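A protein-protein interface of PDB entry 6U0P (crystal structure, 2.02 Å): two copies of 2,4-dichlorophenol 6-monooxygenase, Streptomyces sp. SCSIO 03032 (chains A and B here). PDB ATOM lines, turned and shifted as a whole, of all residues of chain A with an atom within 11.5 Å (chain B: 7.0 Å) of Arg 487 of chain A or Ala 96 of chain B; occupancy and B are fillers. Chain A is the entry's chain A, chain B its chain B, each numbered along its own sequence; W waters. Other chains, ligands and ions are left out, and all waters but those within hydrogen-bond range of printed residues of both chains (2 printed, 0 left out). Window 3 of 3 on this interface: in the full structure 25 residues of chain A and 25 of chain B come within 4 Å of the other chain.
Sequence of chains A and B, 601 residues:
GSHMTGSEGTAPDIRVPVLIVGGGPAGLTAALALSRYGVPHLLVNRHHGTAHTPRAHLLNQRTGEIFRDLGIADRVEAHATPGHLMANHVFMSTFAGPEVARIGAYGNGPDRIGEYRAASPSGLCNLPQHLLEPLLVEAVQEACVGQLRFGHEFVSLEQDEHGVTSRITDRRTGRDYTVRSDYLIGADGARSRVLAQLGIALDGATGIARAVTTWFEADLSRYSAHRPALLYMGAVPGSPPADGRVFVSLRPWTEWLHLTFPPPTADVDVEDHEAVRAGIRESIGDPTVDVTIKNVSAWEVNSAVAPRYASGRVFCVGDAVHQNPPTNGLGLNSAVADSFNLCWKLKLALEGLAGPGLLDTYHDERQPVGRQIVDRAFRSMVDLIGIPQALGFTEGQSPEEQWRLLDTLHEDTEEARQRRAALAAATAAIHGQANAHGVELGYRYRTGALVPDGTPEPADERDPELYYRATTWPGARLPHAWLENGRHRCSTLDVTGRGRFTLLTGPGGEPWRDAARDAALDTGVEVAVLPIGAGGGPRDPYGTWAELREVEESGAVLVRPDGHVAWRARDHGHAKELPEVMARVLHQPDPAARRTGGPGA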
ATOM      1  N   TRP A 482     -23.324   3.681 -22.515  1.00  0.00           N
ATOM      2  CA  TRP A 482     -21.897   3.656 -22.129  1.00  0.00           C
ATOM      3  C   TRP A 482     -21.647   4.689 -21.050  1.00  0.00           C
ATOM      4  O   TRP A 482     -21.911   5.877 -21.269  1.00  0.00           O
ATOM      5  CB  TRP A 482     -20.955   3.857 -23.307  1.00  0.00           C
ATOM      6  CG  TRP A 482     -20.933   2.682 -24.217  1.00  0.00           C
ATOM      7  CD1 TRP A 482     -21.381   2.683 -25.501  1.00  0.00           C
ATOM      8  CD2 TRP A 482     -20.488   1.336 -23.923  1.00  0.00           C
ATOM      9  NE1 TRP A 482     -21.229   1.432 -26.032  1.00  0.00           N
ATOM     10  CE2 TRP A 482     -20.696   0.585 -25.092  1.00  0.00           C
ATOM     11  CE3 TRP A 482     -19.926   0.691 -22.805  1.00  0.00           C
ATOM     12  CZ2 TRP A 482     -20.348  -0.762 -25.190  1.00  0.00           C
ATOM     13  CZ3 TRP A 482     -19.589  -0.643 -22.894  1.00  0.00           C
ATOM     14  CH2 TRP A 482     -19.786  -1.362 -24.081  1.00  0.00           C
ATOM     15  N   LEU A 483     -21.056   4.215 -19.969  1.00  0.00           N
ATOM     16  CA  LEU A 483     -20.595   4.991 -18.824  1.00  0.00           C
ATOM     17  C   LEU A 483     -19.084   4.936 -18.832  1.00  0.00           C
ATOM     18  O   LEU A 483     -18.467   4.097 -19.565  1.00  0.00           O
ATOM     19  CB  LEU A 483     -21.133   4.363 -17.544  1.00  0.00           C
ATOM     20  CG  LEU A 483     -22.644   4.251 -17.414  1.00  0.00           C
ATOM     21  CD1 LEU A 483     -23.013   3.716 -16.048  1.00  0.00           C
ATOM     22  CD2 LEU A 483     -23.319   5.590 -17.655  1.00  0.00           C
ATOM     23  N   GLU A 484     -18.505   5.682 -17.933  1.00  0.00           N
ATOM     24  CA  GLU A 484     -17.051   5.653 -17.717  1.00  0.00           C
ATOM     25  C   GLU A 484     -16.823   5.723 -16.218  1.00  0.00           C
ATOM     26  O   GLU A 484     -17.174   6.774 -15.613  1.00  0.00           O
ATOM     27  CB  GLU A 484     -16.443   6.794 -18.520  1.00  0.00           C
ATOM     28  CG  GLU A 484     -14.967   6.709 -18.644  1.00  0.00           C
ATOM     29  CD  GLU A 484     -14.459   7.809 -19.551  1.00  0.00           C
ATOM     30  OE1 GLU A 484     -14.477   8.982 -19.118  1.00  0.00           O
ATOM     31  OE2 GLU A 484     -14.110   7.487 -20.704  1.00  0.00           O
ATOM     32  N   ASN A 485     -16.243   4.676 -15.637  1.00  0.00           N
ATOM     33  CA  ASN A 485     -15.837   4.704 -14.197  1.00  0.00           C
ATOM     34  C   ASN A 485     -14.328   4.995 -14.065  1.00  0.00           C
ATOM     35  O   ASN A 485     -13.492   4.059 -14.267  1.00  0.00           O
ATOM     36  CB  ASN A 485     -16.313   3.441 -13.481  1.00  0.00           C
ATOM     37  CG  ASN A 485     -16.282   3.583 -11.975  1.00  0.00           C
ATOM     38  OD1 ASN A 485     -16.649   4.637 -11.437  1.00  0.00           O
ATOM     39  ND2 ASN A 485     -15.867   2.520 -11.300  1.00  0.00           N
ATOM     40  N   GLY A 486     -13.955   6.244 -13.734  1.00  0.00           N
ATOM     41  CA  GLY A 486     -12.575   6.717 -13.935  1.00  0.00           C
ATOM     42  C   GLY A 486     -12.286   6.647 -15.420  1.00  0.00           C
ATOM     43  O   GLY A 486     -13.098   7.191 -16.137  1.00  0.00           O
ATOM     44  N   ARG A 487     -11.295   5.874 -15.879  1.00  0.00           N
ATOM     45  CA  ARG A 487     -11.074   5.655 -17.336  1.00  0.00           C
ATOM     46  C   ARG A 487     -11.579   4.282 -17.796  1.00  0.00           C
ATOM     47  O   ARG A 487     -11.220   3.860 -18.909  1.00  0.00           O
ATOM     48  CB  ARG A 487      -9.592   5.859 -17.650  1.00  0.00           C
ATOM     49  CG  ARG A 487      -9.092   7.205 -17.144  1.00  0.00           C
ATOM     50  CD  ARG A 487      -7.674   7.474 -17.592  1.00  0.00           C
ATOM     51  NE  ARG A 487      -7.225   8.790 -17.162  1.00  0.00           N
ATOM     52  CZ  ARG A 487      -6.562   9.045 -16.037  1.00  0.00           C
ATOM     53  NH1 ARG A 487      -6.283   8.082 -15.181  1.00  0.00           N
ATOM     54  NH2 ARG A 487      -6.151  10.270 -15.785  1.00  0.00           N
ATOM     55  N   HIS A 488     -12.399   3.604 -16.999  1.00  0.00           N
ATOM     56  CA  HIS A 488     -12.885   2.246 -17.344  1.00  0.00           C
ATOM     57  C   HIS A 488     -14.230   2.404 -18.029  1.00  0.00           C
ATOM     58  O   HIS A 488     -15.184   2.841 -17.359  1.00  0.00           O
ATOM     59  CB  HIS A 488     -12.946   1.297 -16.113  1.00  0.00           C
ATOM     60  CG  HIS A 488     -13.665   0.019 -16.395  1.00  0.00           C
ATOM     61  ND1 HIS A 488     -13.075  -1.024 -17.122  1.00  0.00           N
ATOM     62  CD2 HIS A 488     -14.919  -0.389 -16.109  1.00  0.00           C
ATOM     63  CE1 HIS A 488     -13.950  -2.002 -17.272  1.00  0.00           C
ATOM     64  NE2 HIS A 488     -15.089  -1.643 -16.671  1.00  0.00           N
ATOM     65  N   ARG A 489     -14.288   2.039 -19.301  1.00  0.00           N
ATOM     66  CA  ARG A 489     -15.532   2.001 -20.106  1.00  0.00           C
ATOM     67  C   ARG A 489     -16.411   0.843 -19.624  1.00  0.00           C
ATOM     68  O   ARG A 489     -15.886  -0.251 -19.444  1.00  0.00           O
ATOM     69  CB  ARG A 489     -15.150   1.862 -21.579  1.00  0.00           C
ATOM     70  CG  ARG A 489     -16.323   1.808 -22.537  1.00  0.00           C
ATOM     71  CD  ARG A 489     -15.695   1.915 -23.917  1.00  0.00           C
ATOM     72  NE  ARG A 489     -16.667   2.104 -24.981  1.00  0.00           N
ATOM     73  CZ  ARG A 489     -17.118   1.140 -25.775  1.00  0.00           C
ATOM     74  NH1 ARG A 489     -16.705  -0.109 -25.615  1.00  0.00           N
ATOM     75  NH2 ARG A 489     -17.980   1.434 -26.733  1.00  0.00           N
ATOM     76  N   CYS A 490     -17.694   1.083 -19.356  1.00  0.00           N
ATOM     77  CA  CYS A 490     -18.612   0.033 -18.868  1.00  0.00           C
ATOM     78  C   CYS A 490     -20.062   0.427 -19.144  1.00  0.00           C
ATOM     79  O   CYS A 490     -20.382   1.614 -19.168  1.00  0.00           O
ATOM     80  CB  CYS A 490     -18.393  -0.205 -17.387  1.00  0.00           C
ATOM     81  SG  CYS A 490     -18.588   1.298 -16.393  1.00  0.00           S
ATOM     82  N   SER A 491     -20.894  -0.542 -19.421  1.00  0.00           N
ATOM     83  CA  SER A 491     -22.336  -0.328 -19.667  1.00  0.00           C
ATOM     84  C   SER A 491     -23.070  -0.067 -18.355  1.00  0.00           C
ATOM     85  O   SER A 491     -22.643  -0.634 -17.318  1.00  0.00           O
ATOM     86  CB  SER A 491     -22.886  -1.537 -20.287  1.00  0.00           C
ATOM     87  OG  SER A 491     -24.271  -1.429 -20.491  1.00  0.00           O
ATOM     88  N   VAL A 495     -22.504  -2.296 -14.454  1.00  0.00           N
ATOM     89  CA  VAL A 495     -22.415  -1.772 -13.073  1.00  0.00           C
ATOM     90  C   VAL A 495     -23.694  -2.130 -12.301  1.00  0.00           C
ATOM     91  O   VAL A 495     -23.794  -1.727 -11.146  1.00  0.00           O
ATOM     92  CB  VAL A 495     -22.133  -0.260 -13.086  1.00  0.00           C
ATOM     93  CG1 VAL A 495     -20.840   0.040 -13.826  1.00  0.00           C
ATOM     94  CG2 VAL A 495     -23.284   0.543 -13.652  1.00  0.00           C
ATOM     95  N   GLY A 536     -19.028  11.551  -7.318  1.00  0.00           N
ATOM     96  CA  GLY A 536     -17.735  10.940  -7.718  1.00  0.00           C
ATOM     97  C   GLY A 536     -17.917   9.574  -8.378  1.00  0.00           C
ATOM     98  O   GLY A 536     -16.921   8.884  -8.592  1.00  0.00           O
ATOM     99  N   GLY A 537     -19.150   9.206  -8.716  1.00  0.00           N
ATOM    100  CA  GLY A 537     -19.496   7.901  -9.302  1.00  0.00           C
ATOM    101  C   GLY A 537     -19.230   7.859 -10.803  1.00  0.00           C
ATOM    102  O   GLY A 537     -18.617   8.752 -11.381  1.00  0.00           O
ATOM    103  N   PRO A 538     -19.697   6.822 -11.516  1.00  0.00           N
ATOM    104  CA  PRO A 538     -19.469   6.761 -12.952  1.00  0.00           C
ATOM    105  C   PRO A 538     -20.017   8.001 -13.672  1.00  0.00           C
ATOM    106  O   PRO A 538     -21.036   8.523 -13.257  1.00  0.00           O
ATOM    107  CB  PRO A 538     -20.278   5.557 -13.433  1.00  0.00           C
ATOM    108  CG  PRO A 538     -20.588   4.753 -12.204  1.00  0.00           C
ATOM    109  CD  PRO A 538     -20.432   5.667 -11.004  1.00  0.00           C
ATOM    110  N   ARG A 539     -19.388   8.383 -14.777  1.00  0.00           N
ATOM    111  CA  ARG A 539     -19.875   9.478 -15.658  1.00  0.00           C
ATOM    112  C   ARG A 539     -20.649   8.892 -16.837  1.00  0.00           C
ATOM    113  O   ARG A 539     -20.469   7.695 -17.176  1.00  0.00           O
ATOM    114  CB  ARG A 539     -18.701  10.333 -16.141  1.00  0.00           C
ATOM    115  CG  ARG A 539     -17.675  10.645 -15.059  1.00  0.00           C
ATOM    116  CD  ARG A 539     -16.639  11.623 -15.565  1.00  0.00           C
ATOM    117  NE  ARG A 539     -17.151  12.394 -16.691  1.00  0.00           N
ATOM    118  CZ  ARG A 539     -16.837  12.204 -17.973  1.00  0.00           C
ATOM    119  NH1 ARG A 539     -15.976  11.258 -18.325  1.00  0.00           N
ATOM    120  NH2 ARG A 539     -17.387  12.975 -18.899  1.00  0.00           N
ATOM    121  N   ASP A 540     -21.479   9.734 -17.438  1.00  0.00           N
ATOM    122  CA  ASP A 540     -22.346   9.482 -18.611  1.00  0.00           C
ATOM    123  C   ASP A 540     -21.787  10.332 -19.767  1.00  0.00           C
ATOM    124  O   ASP A 540     -22.329  11.382 -20.076  1.00  0.00           O
ATOM    125  CB  ASP A 540     -23.788   9.809 -18.195  1.00  0.00           C
ATOM    126  CG  ASP A 540     -24.824   9.803 -19.301  1.00  0.00           C
ATOM    127  OD1 ASP A 540     -24.576   9.082 -20.308  1.00  0.00           O
ATOM    128  OD2 ASP A 540     -25.899  10.517 -19.148  1.00  0.00           O
ATOM    129  N   PRO A 541     -20.678   9.951 -20.445  1.00  0.00           N
ATOM    130  CA  PRO A 541     -19.905  10.915 -21.236  1.00  0.00           C
ATOM    131  C   PRO A 541     -20.651  11.564 -22.395  1.00  0.00           C
ATOM    132  O   PRO A 541     -20.257  12.665 -22.758  1.00  0.00           O
ATOM    133  CB  PRO A 541     -18.771  10.086 -21.859  1.00  0.00           C
ATOM    134  CG  PRO A 541     -18.668   8.924 -20.909  1.00  0.00           C
ATOM    135  CD  PRO A 541     -20.107   8.598 -20.544  1.00  0.00           C
ATOM    136  N   TYR A 542     -21.608  10.853 -22.977  1.00  0.00           N
ATOM    137  CA  TYR A 542     -22.358  11.305 -24.175  1.00  0.00           C
ATOM    138  C   TYR A 542     -23.652  11.944 -23.700  1.00  0.00           C
ATOM    139  O   TYR A 542     -24.245  12.592 -24.512  1.00  0.00           O
ATOM    140  CB  TYR A 542     -22.694  10.174 -25.155  1.00  0.00           C
ATOM    141  CG  TYR A 542     -21.483   9.432 -25.656  1.00  0.00           C
ATOM    142  CD1 TYR A 542     -20.699   9.921 -26.689  1.00  0.00           C
ATOM    143  CD2 TYR A 542     -21.038   8.301 -24.995  1.00  0.00           C
ATOM    144  CE1 TYR A 542     -19.548   9.251 -27.096  1.00  0.00           C
ATOM    145  CE2 TYR A 542     -19.909   7.599 -25.407  1.00  0.00           C
ATOM    146  CZ  TYR A 542     -19.159   8.068 -26.468  1.00  0.00           C
ATOM    147  OH  TYR A 542     -18.004   7.387 -26.781  1.00  0.00           O
ATOM    148  N   MET B  92     -11.944  18.395 -23.064  1.00  0.00           N
ATOM    149  CA  MET B  92     -11.382  17.985 -21.761  1.00  0.00           C
ATOM    150  C   MET B  92     -10.680  19.178 -21.098  1.00  0.00           C
ATOM    151  O   MET B  92     -10.662  20.297 -21.686  1.00  0.00           O
ATOM    152  CB  MET B  92     -10.405  16.835 -21.990  1.00  0.00           C
ATOM    153  CG  MET B  92      -9.218  17.248 -22.809  1.00  0.00           C
ATOM    154  SD  MET B  92      -8.337  15.844 -23.438  1.00  0.00           S
ATOM    155  CE  MET B  92      -6.871  16.650 -24.082  1.00  0.00           C
ATOM    156  N   SER B  93     -10.213  18.971 -19.872  1.00  0.00           N
ATOM    157  CA  SER B  93      -9.300  19.886 -19.152  1.00  0.00           C
ATOM    158  C   SER B  93      -7.878  19.609 -19.655  1.00  0.00           C
ATOM    159  O   SER B  93      -7.547  19.985 -20.824  1.00  0.00           O
ATOM    160  CB  SER B  93      -9.481  19.732 -17.647  1.00  0.00           C
ATOM    161  OG  SER B  93      -9.115  18.417 -17.198  1.00  0.00           O
ATOM    162  N   THR B  94      -7.031  18.988 -18.847  1.00  0.00           N
ATOM    163  CA  THR B  94      -5.765  18.407 -19.345  1.00  0.00           C
ATOM    164  C   THR B  94      -6.100  17.033 -19.940  1.00  0.00           C
ATOM    165  O   THR B  94      -7.202  16.527 -19.685  1.00  0.00           O
ATOM    166  CB  THR B  94      -4.715  18.253 -18.240  1.00  0.00           C
ATOM    167  OG1 THR B  94      -5.288  17.446 -17.207  1.00  0.00           O
ATOM    168  CG2 THR B  94      -4.220  19.582 -17.719  1.00  0.00           C
ATOM    169  N   PHE B  95      -5.143  16.420 -20.611  1.00  0.00           N
ATOM    170  CA  PHE B  95      -5.291  15.069 -21.210  1.00  0.00           C
ATOM    171  C   PHE B  95      -5.447  14.045 -20.076  1.00  0.00           C
ATOM    172  O   PHE B  95      -6.314  13.147 -20.178  1.00  0.00           O
ATOM    173  CB  PHE B  95      -4.117  14.815 -22.157  1.00  0.00           C
ATOM    174  CG  PHE B  95      -4.487  14.133 -23.443  1.00  0.00           C
ATOM    175  CD1 PHE B  95      -3.734  14.331 -24.579  1.00  0.00           C
ATOM    176  CD2 PHE B  95      -5.576  13.282 -23.508  1.00  0.00           C
ATOM    177  CE1 PHE B  95      -4.072  13.691 -25.763  1.00  0.00           C
ATOM    178  CE2 PHE B  95      -5.902  12.634 -24.687  1.00  0.00           C
ATOM    179  CZ  PHE B  95      -5.159  12.847 -25.815  1.00  0.00           C
ATOM    180  N   ALA B  96      -4.707  14.252 -18.980  1.00  0.00           N
ATOM    181  CA  ALA B  96      -4.677  13.402 -17.769  1.00  0.00           C
ATOM    182  C   ALA B  96      -5.777  13.787 -16.784  1.00  0.00           C
ATOM    183  O   ALA B  96      -5.993  13.031 -15.853  1.00  0.00           O
ATOM    184  CB  ALA B  96      -3.342  13.495 -17.093  1.00  0.00           C
ATOM    185  N   GLY B  97      -6.459  14.906 -16.988  1.00  0.00           N
ATOM    186  CA  GLY B  97      -7.436  15.413 -16.010  1.00  0.00           C
ATOM    187  C   GLY B  97      -8.854  15.016 -16.395  1.00  0.00           C
ATOM    188  O   GLY B  97      -9.084  14.204 -17.295  1.00  0.00           O
ATOM    189  N   PRO B  98      -9.858  15.575 -15.710  1.00  0.00           N
ATOM    190  CA  PRO B  98     -11.246  15.285 -16.046  1.00  0.00           C
ATOM    191  C   PRO B  98     -11.623  15.814 -17.430  1.00  0.00           C
ATOM    192  O   PRO B  98     -11.061  16.824 -17.887  1.00  0.00           O
ATOM    193  CB  PRO B  98     -12.086  15.998 -14.978  1.00  0.00           C
ATOM    194  CG  PRO B  98     -11.134  17.003 -14.357  1.00  0.00           C
ATOM    195  CD  PRO B  98      -9.726  16.452 -14.535  1.00  0.00           C
ATOM    196  N   LEU B 220       0.570   8.509 -25.263  1.00  0.00           N
ATOM    197  CA  LEU B 220      -0.582   8.998 -24.483  1.00  0.00           C
ATOM    198  C   LEU B 220      -1.716   7.952 -24.512  1.00  0.00           C
ATOM    199  O   LEU B 220      -2.869   8.337 -24.263  1.00  0.00           O
ATOM    200  CB  LEU B 220      -0.991  10.369 -25.034  1.00  0.00           C
ATOM    201  CG  LEU B 220       0.040  11.492 -24.861  1.00  0.00           C
ATOM    202  CD1 LEU B 220      -0.192  12.637 -25.831  1.00  0.00           C
ATOM    203  CD2 LEU B 220       0.035  12.004 -23.441  1.00  0.00           C
ATOM    204  N   ARG B 222      -2.681   5.726 -22.398  1.00  0.00           N
ATOM    205  CA  ARG B 222      -3.402   5.713 -21.102  1.00  0.00           C
ATOM    206  C   ARG B 222      -4.515   6.768 -21.055  1.00  0.00           C
ATOM    207  O   ARG B 222      -5.469   6.621 -20.261  1.00  0.00           O
ATOM    208  CB  ARG B 222      -2.366   5.973 -20.015  1.00  0.00           C
ATOM    209  CG  ARG B 222      -2.934   6.004 -18.614  1.00  0.00           C
ATOM    210  CD  ARG B 222      -1.794   5.796 -17.637  1.00  0.00           C
ATOM    211  NE  ARG B 222      -2.374   5.552 -16.327  1.00  0.00           N
ATOM    212  CZ  ARG B 222      -1.702   5.591 -15.177  1.00  0.00           C
ATOM    213  NH1 ARG B 222      -0.405   5.852 -15.189  1.00  0.00           N
ATOM    214  NH2 ARG B 222      -2.325   5.364 -14.024  1.00  0.00           N
ATOM    215  N   TYR B 223      -4.398   7.845 -21.823  1.00  0.00           N
ATOM    216  CA  TYR B 223      -5.381   8.955 -21.769  1.00  0.00           C
ATOM    217  C   TYR B 223      -6.258   8.970 -23.028  1.00  0.00           C
ATOM    218  O   TYR B 223      -7.174   9.823 -23.073  1.00  0.00           O
ATOM    219  CB  TYR B 223      -4.656  10.277 -21.510  1.00  0.00           C
ATOM    220  CG  TYR B 223      -3.761  10.245 -20.299  1.00  0.00           C
ATOM    221  CD1 TYR B 223      -4.278   9.920 -19.050  1.00  0.00           C
ATOM    222  CD2 TYR B 223      -2.408  10.520 -20.395  1.00  0.00           C
ATOM    223  CE1 TYR B 223      -3.472   9.866 -17.925  1.00  0.00           C
ATOM    224  CE2 TYR B 223      -1.584  10.481 -19.279  1.00  0.00           C
ATOM    225  CZ  TYR B 223      -2.121  10.144 -18.044  1.00  0.00           C
ATOM    226  OH  TYR B 223      -1.351  10.095 -16.928  1.00  0.00           O
ATOM    227  N   SER B 224      -6.066   8.064 -23.992  1.00  0.00           N
ATOM    228  CA  SER B 224      -6.815   8.166 -25.273  1.00  0.00           C
ATOM    229  C   SER B 224      -7.530   6.889 -25.679  1.00  0.00           C
ATOM    230  O   SER B 224      -8.568   6.995 -26.420  1.00  0.00           O
ATOM    231  CB  SER B 224      -5.914   8.713 -26.385  1.00  0.00           C
ATOM    232  OG  SER B 224      -4.637   8.121 -26.366  1.00  0.00           O
ATOM    233  N   HIS B 226      -9.286   4.516 -24.387  1.00  0.00           N
ATOM    234  CA  HIS B 226     -10.641   4.253 -23.863  1.00  0.00           C
ATOM    235  C   HIS B 226     -11.630   5.290 -24.437  1.00  0.00           C
ATOM    236  O   HIS B 226     -12.842   5.119 -24.246  1.00  0.00           O
ATOM    237  CB  HIS B 226     -10.581   4.236 -22.333  1.00  0.00           C
ATOM    238  CG  HIS B 226     -10.304   5.588 -21.764  1.00  0.00           C
ATOM    239  ND1 HIS B 226      -9.011   6.112 -21.669  1.00  0.00           N
ATOM    240  CD2 HIS B 226     -11.140   6.546 -21.304  1.00  0.00           C
ATOM    241  CE1 HIS B 226      -9.088   7.335 -21.164  1.00  0.00           C
ATOM    242  NE2 HIS B 226     -10.378   7.617 -20.929  1.00  0.00           N
ATOM    243  N   ARG B 227     -11.167   6.281 -25.202  1.00  0.00           N
ATOM    244  CA  ARG B 227     -12.070   7.281 -25.856  1.00  0.00           C
ATOM    245  C   ARG B 227     -11.464   7.714 -27.187  1.00  0.00           C
ATOM    246  O   ARG B 227     -11.007   8.862 -27.345  1.00  0.00           O
ATOM    247  CB  ARG B 227     -12.282   8.486 -24.934  1.00  0.00           C
ATOM    248  CG  ARG B 227     -10.991   8.960 -24.283  1.00  0.00           C
ATOM    249  CD  ARG B 227     -11.193  10.219 -23.476  1.00  0.00           C
ATOM    250  NE  ARG B 227      -9.918  10.700 -23.004  1.00  0.00           N
ATOM    251  CZ  ARG B 227      -9.758  11.785 -22.267  1.00  0.00           C
ATOM    252  NH1 ARG B 227     -10.821  12.458 -21.845  1.00  0.00           N
ATOM    253  NH2 ARG B 227      -8.539  12.115 -21.893  1.00  0.00           N
ATOM    254  N   SER B 283      -0.301  20.864 -21.155  1.00  0.00           N
ATOM    255  CA  SER B 283      -1.573  20.433 -21.813  1.00  0.00           C
ATOM    256  C   SER B 283      -1.891  18.979 -21.408  1.00  0.00           C
ATOM    257  O   SER B 283      -3.049  18.662 -21.125  1.00  0.00           O
ATOM    258  CB  SER B 283      -1.500  20.560 -23.323  1.00  0.00           C
ATOM    259  OG  SER B 283      -1.240  21.898 -23.737  1.00  0.00           O
ATOM    260  N   ILE B 284      -0.865  18.146 -21.322  1.00  0.00           N
ATOM    261  CA  ILE B 284      -0.990  16.703 -20.985  1.00  0.00           C
ATOM    262  C   ILE B 284      -1.346  16.589 -19.506  1.00  0.00           C
ATOM    263  O   ILE B 284      -2.310  15.874 -19.208  1.00  0.00           O
ATOM    264  CB  ILE B 284       0.313  15.990 -21.389  1.00  0.00           C
ATOM    265  CG1 ILE B 284       0.427  15.974 -22.913  1.00  0.00           C
ATOM    266  CG2 ILE B 284       0.407  14.610 -20.778  1.00  0.00           C
ATOM    267  CD1 ILE B 284       1.740  15.437 -23.447  1.00  0.00           C
ATOM    268  N   GLY B 285      -0.653  17.343 -18.641  1.00  0.00           N
ATOM    269  CA  GLY B 285      -0.908  17.424 -17.186  1.00  0.00           C
ATOM    270  C   GLY B 285      -0.369  16.224 -16.422  1.00  0.00           C
ATOM    271  O   GLY B 285      -0.948  15.900 -15.399  1.00  0.00           O
ATOM    272  N   ASP B 286       0.675  15.560 -16.923  1.00  0.00           N
ATOM    273  CA  ASP B 286       1.284  14.334 -16.335  1.00  0.00           C
ATOM    274  C   ASP B 286       2.771  14.397 -16.656  1.00  0.00           C
ATOM    275  O   ASP B 286       3.206  13.964 -17.732  1.00  0.00           O
ATOM    276  CB  ASP B 286       0.645  13.036 -16.853  1.00  0.00           C
ATOM    277  CG  ASP B 286       1.331  11.739 -16.422  1.00  0.00           C
ATOM    278  OD1 ASP B 286       2.248  11.794 -15.582  1.00  0.00           O
ATOM    279  OD2 ASP B 286       0.946  10.667 -16.951  1.00  0.00           O
HETATM  280  O   HOH W   1     -14.750   5.820 -22.529  1.00  0.00           O
HETATM  281  O   HOH W   2      -7.768  11.411 -18.654  1.00  0.00           O
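NH2 of Arg 487 of chain A lies within hydrogen-bond range of O of Ala 96 of chain B (2.8 Å).
The side-chain carboxylate (OE1) of Glu 484 of chain A lies within salt-bridge range of the guanidinium group (NH1) of Arg 539 of chain A, at 2.8 Å. The backbone NH of Ala 96 of chain B sits at hydrogen-bond distance from the backbone carbonyl oxygen of Ile 284 of chain B (2.9 Å). The backbone carbonyl oxygen (O) of Tyr 223 of chain B is in hydrogen-bond range of the guanidinium group (NE) of Arg 227 of chain B (2.9 Å).
Among the printed residues, pairs that only touch across the chains: Glu 484 of chain A with His 226 of chain B (3.2 Å), Arg 487 of chain A with Arg 222 of chain B (3.6 Å), Arg 487 of chain A with Tyr 223 of chain B (3.5 Å) and Arg 487 of chain A with His 226 of chain B (3.5 Å).
Arg 487 of chain A touches just these residues of chain B: Ala 96, Arg 222, Tyr 223 and His 226. Ala 96 of chain B touches just one residue of chain A: Arg 487. No residue of chain A comes within 4 Å of Ser 93 of chain B. No residue of chain A comes within 4 Å of Phe 95 of chain B. No residue of chain A comes within 4 Å of Pro 98 of chain B. Of the printed residues of chain A, Arg 222 of chain B touches Arg 487 (3.6 Å). Of chain A, only Arg 487 comes within 4 Å of Tyr 223 of chain B. No residue of chain A comes within 4 Å of Asp 286 of chain B. Of the printed residues of chain B, Glu 484 of chain A touches His 226 (3.2 Å). Asp 540 of chain A touches none of the printed residues of chain B. The nearest residue of chain B that does not touch Arg 487 of chain A is Gly 97 of chain B (4.8 Å). The nearest residue of chain A that does not touch Ala 96 of chain B is Gly 486 of chain A (9.0 Å). The nearest printed residue of chain B that does not touch Glu 484 of chain A is Arg 227 of chain B (4.7 Å).
Of the 17 printed residues of chain B, 4 touch a printed residue of chain A. Hydrophobic or aromatic side chains of chain B within 4 Å of the printed part of chain A: Tyr 223 and His 226.
No position is printed for both chains. Of the 5 pairs that touch across the chains among the printed residues, none has its exchanged pair printed and touching as well.
Water W1 bridges the side-chain carboxylate (OE2) of Glu 484 of chain A (2.6 Å) and the backbone carbonyl oxygen (O) of His 226 of chain B (2.7 Å). Water W2 lies within hydrogen-bond range of the backbone carbonyl oxygen (O) of Phe 95 of chain B (2.7 Å), the guanidinium group (NE) of Arg 487 of chain A (3.1 Å), the backbone carbonyl oxygen (O) of Gly 97 of chain B (3.4 Å) and the guanidinium group (NH2) of Arg 227 of chain B (3.4 Å).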
